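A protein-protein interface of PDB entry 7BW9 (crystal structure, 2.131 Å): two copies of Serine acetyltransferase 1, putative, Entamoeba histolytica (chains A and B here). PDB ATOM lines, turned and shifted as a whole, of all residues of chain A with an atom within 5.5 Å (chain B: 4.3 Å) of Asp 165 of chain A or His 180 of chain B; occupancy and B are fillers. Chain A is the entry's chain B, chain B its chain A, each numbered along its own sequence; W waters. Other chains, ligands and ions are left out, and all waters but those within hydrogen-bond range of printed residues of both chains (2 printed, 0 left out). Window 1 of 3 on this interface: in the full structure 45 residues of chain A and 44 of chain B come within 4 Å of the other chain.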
ATOM      1  N   ARG A 152      12.977  -6.701  11.254  1.00  0.00           N
ATOM      2  CA  ARG A 152      11.943  -7.151  10.327  1.00  0.00           C
ATOM      3  C   ARG A 152      12.519  -8.113   9.300  1.00  0.00           C
ATOM      4  O   ARG A 152      11.893  -9.127   8.968  1.00  0.00           O
ATOM      5  CB  ARG A 152      11.292  -5.946   9.639  1.00  0.00           C
ATOM      6  CG  ARG A 152      10.208  -6.292   8.611  1.00  0.00           C
ATOM      7  CD  ARG A 152       9.003  -6.992   9.263  1.00  0.00           C
ATOM      8  NE  ARG A 152       8.038  -7.489   8.277  1.00  0.00           N
ATOM      9  CZ  ARG A 152       7.053  -6.748   7.770  1.00  0.00           C
ATOM     10  NH1 ARG A 152       6.921  -5.475   8.138  1.00  0.00           N
ATOM     11  NH2 ARG A 152       6.205  -7.266   6.885  1.00  0.00           N
ATOM     12  N   GLU A 156      11.442 -11.898   8.584  1.00  0.00           N
ATOM     13  CA  GLU A 156      11.125 -12.389   7.243  1.00  0.00           C
ATOM     14  C   GLU A 156      12.009 -13.564   6.833  1.00  0.00           C
ATOM     15  O   GLU A 156      11.579 -14.404   6.034  1.00  0.00           O
ATOM     16  CB  GLU A 156      11.242 -11.264   6.217  1.00  0.00           C
ATOM     17  CG  GLU A 156      10.150 -10.218   6.372  1.00  0.00           C
ATOM     18  CD  GLU A 156       8.719 -10.757   6.146  1.00  0.00           C
ATOM     19  OE1 GLU A 156       8.532 -11.829   5.519  1.00  0.00           O
ATOM     20  OE2 GLU A 156       7.770 -10.091   6.607  1.00  0.00           O
ATOM     21  N   HIS A 159      10.327 -16.354   8.573  1.00  0.00           N
ATOM     22  CA  HIS A 159       9.056 -16.467   7.860  1.00  0.00           C
ATOM     23  C   HIS A 159       9.206 -17.334   6.616  1.00  0.00           C
ATOM     24  O   HIS A 159       8.402 -18.240   6.372  1.00  0.00           O
ATOM     25  CB  HIS A 159       8.576 -15.059   7.488  1.00  0.00           C
ATOM     26  CG  HIS A 159       7.261 -15.017   6.780  1.00  0.00           C
ATOM     27  ND1 HIS A 159       6.833 -13.905   6.083  1.00  0.00           N
ATOM     28  CD2 HIS A 159       6.263 -15.925   6.687  1.00  0.00           C
ATOM     29  CE1 HIS A 159       5.638 -14.138   5.571  1.00  0.00           C
ATOM     30  NE2 HIS A 159       5.268 -15.355   5.926  1.00  0.00           N
ATOM     31  N   GLY A 163       6.992 -20.462   7.097  1.00  0.00           N
ATOM     32  CA  GLY A 163       5.652 -20.025   6.779  1.00  0.00           C
ATOM     33  C   GLY A 163       4.904 -19.370   7.924  1.00  0.00           C
ATOM     34  O   GLY A 163       3.700 -19.128   7.796  1.00  0.00           O
ATOM     35  N   ILE A 164       5.580 -19.079   9.037  1.00  0.00           N
ATOM     36  CA  ILE A 164       4.997 -18.387  10.182  1.00  0.00           C
ATOM     37  C   ILE A 164       5.489 -16.949  10.170  1.00  0.00           C
ATOM     38  O   ILE A 164       6.703 -16.699  10.143  1.00  0.00           O
ATOM     39  CB  ILE A 164       5.378 -19.073  11.504  1.00  0.00           C
ATOM     40  CG1 ILE A 164       4.922 -20.537  11.531  1.00  0.00           C
ATOM     41  CG2 ILE A 164       4.872 -18.269  12.690  1.00  0.00           C
ATOM     42  CD1 ILE A 164       5.566 -21.341  12.683  1.00  0.00           C
ATOM     43  N   ASP A 165       4.560 -16.005  10.198  1.00  0.00           N
ATOM     44  CA  ASP A 165       4.854 -14.583  10.025  1.00  0.00           C
ATOM     45  C   ASP A 165       4.556 -13.856  11.332  1.00  0.00           C
ATOM     46  O   ASP A 165       3.396 -13.557  11.644  1.00  0.00           O
ATOM     47  CB  ASP A 165       4.042 -14.004   8.865  1.00  0.00           C
ATOM     48  CG  ASP A 165       4.453 -12.570   8.504  1.00  0.00           C
ATOM     49  OD1 ASP A 165       5.353 -11.996   9.160  1.00  0.00           O
ATOM     50  OD2 ASP A 165       3.889 -12.015   7.533  1.00  0.00           O
ATOM     51  N   ILE A 166       5.597 -13.560  12.094  1.00  0.00           N
ATOM     52  CA  ILE A 166       5.448 -12.830  13.341  1.00  0.00           C
ATOM     53  C   ILE A 166       6.263 -11.554  13.253  1.00  0.00           C
ATOM     54  O   ILE A 166       7.476 -11.601  13.005  1.00  0.00           O
ATOM     55  CB  ILE A 166       5.869 -13.663  14.559  1.00  0.00           C
ATOM     56  CG1 ILE A 166       5.085 -14.978  14.585  1.00  0.00           C
ATOM     57  CG2 ILE A 166       5.634 -12.843  15.830  1.00  0.00           C
ATOM     58  CD1 ILE A 166       5.316 -15.832  15.835  1.00  0.00           C
ATOM     59  N   HIS A 167       5.611 -10.422  13.492  1.00  0.00           N
ATOM     60  CA  HIS A 167       6.313  -9.154  13.465  1.00  0.00           C
ATOM     61  C   HIS A 167       7.266  -9.041  14.658  1.00  0.00           C
ATOM     62  O   HIS A 167       6.940  -9.483  15.765  1.00  0.00           O
ATOM     63  CB  HIS A 167       5.305  -8.008  13.471  1.00  0.00           C
ATOM     64  CG  HIS A 167       5.895  -6.684  13.111  1.00  0.00           C
ATOM     65  ND1 HIS A 167       6.576  -5.903  14.022  1.00  0.00           N
ATOM     66  CD2 HIS A 167       5.911  -6.001  11.943  1.00  0.00           C
ATOM     67  CE1 HIS A 167       6.990  -4.796  13.429  1.00  0.00           C
ATOM     68  NE2 HIS A 167       6.603  -4.832  12.166  1.00  0.00           N
ATOM     69  N   VAL A 184       0.268 -18.736   9.841  1.00  0.00           N
ATOM     70  CA  VAL A 184       0.068 -17.890  11.016  1.00  0.00           C
ATOM     71  C   VAL A 184       0.645 -16.505  10.758  1.00  0.00           C
ATOM     72  O   VAL A 184       1.800 -16.358  10.326  1.00  0.00           O
ATOM     73  CB  VAL A 184       0.710 -18.537  12.256  1.00  0.00           C
ATOM     74  CG1 VAL A 184       0.873 -17.528  13.397  1.00  0.00           C
ATOM     75  CG2 VAL A 184      -0.095 -19.735  12.705  1.00  0.00           C
ATOM     76  N   VAL A 185      -0.143 -15.479  11.057  1.00  0.00           N
ATOM     77  CA  VAL A 185       0.271 -14.091  10.909  1.00  0.00           C
ATOM     78  C   VAL A 185      -0.065 -13.361  12.199  1.00  0.00           C
ATOM     79  O   VAL A 185      -1.217 -13.394  12.654  1.00  0.00           O
ATOM     80  CB  VAL A 185      -0.432 -13.398   9.725  1.00  0.00           C
ATOM     81  CG1 VAL A 185      -0.127 -11.901   9.736  1.00  0.00           C
ATOM     82  CG2 VAL A 185      -0.073 -14.042   8.385  1.00  0.00           C
ATOM     83  N   ILE A 186       0.920 -12.670  12.766  1.00  0.00           N
ATOM     84  CA  ILE A 186       0.733 -11.946  14.012  1.00  0.00           C
ATOM     85  C   ILE A 186       1.358 -10.571  13.848  1.00  0.00           C
ATOM     86  O   ILE A 186       2.557 -10.461  13.582  1.00  0.00           O
ATOM     87  CB  ILE A 186       1.338 -12.688  15.212  1.00  0.00           C
ATOM     88  CG1 ILE A 186       0.774 -14.113  15.300  1.00  0.00           C
ATOM     89  CG2 ILE A 186       1.052 -11.918  16.469  1.00  0.00           C
ATOM     90  CD1 ILE A 186       1.280 -14.955  16.494  1.00  0.00           C
ATOM     91  N   GLY A 187       0.561  -9.534  14.021  1.00  0.00           N
ATOM     92  CA  GLY A 187       0.976  -8.213  13.616  1.00  0.00           C
ATOM     93  C   GLY A 187       1.792  -7.463  14.656  1.00  0.00           C
ATOM     94  O   GLY A 187       1.927  -7.863  15.808  1.00  0.00           O
ATOM     95  N   PRO B 128       7.901 -10.527   1.047  1.00  0.00           N
ATOM     96  CA  PRO B 128       7.704 -11.669   0.133  1.00  0.00           C
ATOM     97  C   PRO B 128       6.734 -11.382  -0.997  1.00  0.00           C
ATOM     98  O   PRO B 128       6.844 -12.012  -2.056  1.00  0.00           O
ATOM     99  CB  PRO B 128       7.167 -12.780   1.047  1.00  0.00           C
ATOM    100  CG  PRO B 128       6.561 -12.049   2.216  1.00  0.00           C
ATOM    101  CD  PRO B 128       7.420 -10.810   2.409  1.00  0.00           C
ATOM    102  N   ILE B 178       0.529  -7.840  -2.222  1.00  0.00           N
ATOM    103  CA  ILE B 178       0.221  -8.985  -1.370  1.00  0.00           C
ATOM    104  C   ILE B 178       0.896  -8.745  -0.027  1.00  0.00           C
ATOM    105  O   ILE B 178       2.127  -8.622   0.036  1.00  0.00           O
ATOM    106  CB  ILE B 178       0.695 -10.307  -1.997  1.00  0.00           C
ATOM    107  CG1 ILE B 178      -0.110 -10.624  -3.253  1.00  0.00           C
ATOM    108  CG2 ILE B 178       0.584 -11.461  -0.999  1.00  0.00           C
ATOM    109  CD1 ILE B 178       0.401 -11.819  -4.006  1.00  0.00           C
ATOM    110  N   ASP B 179       0.100  -8.639   1.036  1.00  0.00           N
ATOM    111  CA  ASP B 179       0.617  -8.504   2.397  1.00  0.00           C
ATOM    112  C   ASP B 179       0.640  -9.875   3.056  1.00  0.00           C
ATOM    113  O   ASP B 179      -0.356 -10.603   3.001  1.00  0.00           O
ATOM    114  CB  ASP B 179      -0.227  -7.535   3.233  1.00  0.00           C
ATOM    115  CG  ASP B 179       0.545  -6.956   4.438  1.00  0.00           C
ATOM    116  OD1 ASP B 179       1.740  -7.293   4.628  1.00  0.00           O
ATOM    117  OD2 ASP B 179      -0.050  -6.158   5.203  1.00  0.00           O
ATOM    118  N   HIS B 180       1.786 -10.225   3.658  1.00  0.00           N
ATOM    119  CA  HIS B 180       2.008 -11.499   4.345  1.00  0.00           C
ATOM    120  C   HIS B 180       2.067 -12.648   3.343  1.00  0.00           C
ATOM    121  O   HIS B 180       3.139 -13.219   3.130  1.00  0.00           O
ATOM    122  CB  HIS B 180       0.939 -11.758   5.417  1.00  0.00           C
ATOM    123  CG  HIS B 180       0.824 -10.659   6.434  1.00  0.00           C
ATOM    124  ND1 HIS B 180       1.889 -10.241   7.205  1.00  0.00           N
ATOM    125  CD2 HIS B 180      -0.231  -9.887   6.803  1.00  0.00           C
ATOM    126  CE1 HIS B 180       1.495  -9.260   8.003  1.00  0.00           C
ATOM    127  NE2 HIS B 180       0.214  -9.023   7.778  1.00  0.00           N
ATOM    128  N   GLY B 181       0.932 -13.033   2.755  1.00  0.00           N
ATOM    129  CA  GLY B 181       0.943 -13.811   1.536  1.00  0.00           C
ATOM    130  C   GLY B 181       0.958 -15.325   1.668  1.00  0.00           C
ATOM    131  O   GLY B 181       0.589 -16.006   0.699  1.00  0.00           O
ATOM    132  N   VAL B 182       1.396 -15.892   2.803  1.00  0.00           N
ATOM    133  CA  VAL B 182       1.447 -17.354   2.905  1.00  0.00           C
ATOM    134  C   VAL B 182       0.046 -17.913   2.717  1.00  0.00           C
ATOM    135  O   VAL B 182      -0.927 -17.395   3.279  1.00  0.00           O
ATOM    136  CB  VAL B 182       2.042 -17.817   4.247  1.00  0.00           C
ATOM    137  CG1 VAL B 182       1.829 -19.313   4.418  1.00  0.00           C
ATOM    138  CG2 VAL B 182       3.537 -17.530   4.328  1.00  0.00           C
ATOM    139  N   GLN B 200      -3.006 -12.864   3.391  1.00  0.00           N
ATOM    140  CA  GLN B 200      -2.663 -14.275   3.560  1.00  0.00           C
ATOM    141  C   GLN B 200      -3.877 -15.176   3.360  1.00  0.00           C
ATOM    142  O   GLN B 200      -5.015 -14.783   3.623  1.00  0.00           O
ATOM    143  CB  GLN B 200      -2.071 -14.523   4.954  1.00  0.00           C
ATOM    144  CG  GLN B 200      -2.958 -14.127   6.143  1.00  0.00           C
ATOM    145  CD  GLN B 200      -2.880 -12.653   6.479  1.00  0.00           C
ATOM    146  OE1 GLN B 200      -2.443 -11.839   5.658  1.00  0.00           O
ATOM    147  NE2 GLN B 200      -3.316 -12.291   7.687  1.00  0.00           N
HETATM  148  O   HOH W   1       2.252 -14.815   5.558  1.00  0.00           O
HETATM  149  O   HOH W   2       3.303  -6.465   6.534  1.00  0.00           O
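No position is printed for both chains.
Of the 7 pairs that touch across the chains among the printed residues, none has its exchanged pair printed and touching as well.
ND1 of His 180 of chain B lies within hydrogen-bond range of OD2 of Asp 165 of chain A (2.7 Å).
Printed residues of chain B within 4 Å of His 159 of chain A: His 180 (3.6 Å) and Val 182 (3.2 Å).
Printed residues of chain B within 4 Å of Gly 163 of chain A: Val 182.
Of chain B, only His 180 comes within 4 Å of Asp 165 of chain A.
Of the printed residues of chain A, Pro 128 of chain B touches Glu 156.
Of the printed residues of chain A, Val 182 of chain B touches His 159 and Gly 163.
Of the printed residues of chain A, Gln 200 of chain B touches Val 185 (3.7 Å).
The nearest printed residue of chain B that does not touch Asp 165 of chain A is Gly 181 of chain B (5.7 Å).
Of the 7 printed residues of chain B, 4 touch a printed residue of chain A.
Printed residues of chain B that touch a printed residue of chain A: Pro 128, His 180, Val 182 and Gln 200.
Hydrophobic or aromatic side chains of chain B within 4 Å of the printed part of chain A: Pro 128, His 180 and Val 182.
Hydrophobic or aromatic side chains of chain A that line the printed part of chain B: His 159 and Val 185.
Among the printed residues, no Asp or Glu carboxylate lies within 4 Å of a Lys or Arg side-chain nitrogen of the other chain.
Water W2 bridges OD1 of Asp 179 of chain B (2.6 Å) and NH2 of Arg 152 of chain A (3.0 Å).
Water W1 lies within hydrogen-bond range of O of His 180 of chain B (3.0 Å), N of Val 182 of chain B (3.1 Å) and NE2 of His 159 of chain A (3.1 Å).
ND1 of His 159 of chain A lies within hydrogen-bond range of OE1 of Glu 156 of chain A (2.7 Å).
The backbone NH (N) of Asp 165 of chain A is in hydrogen-bond range of the backbone carbonyl oxygen (O) of Val 184 of chain A (2.8 Å).
N of Ile 186 of chain A sits at hydrogen-bond distance from O of Asp 165 of chain A, at 2.9 Å.
The side-chain carboxylate (OE2) of Glu 156 of chain A is in salt-bridge range of the guanidinium group (NE) of Arg 152 of chain A (3.1 Å).
Among the printed residues, pairs that only touch across the chains: His 159 of chain A with Val 182 of chain B, Glu 156 of chain A with Pro 128 of chain B, Val 185 of chain A with His 180 of chain B, His 159 of chain A with His 180 of chain B, Val 185 of chain A with Gln 200 of chain B and Gly 163 of chain A with Val 182 of chain B.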
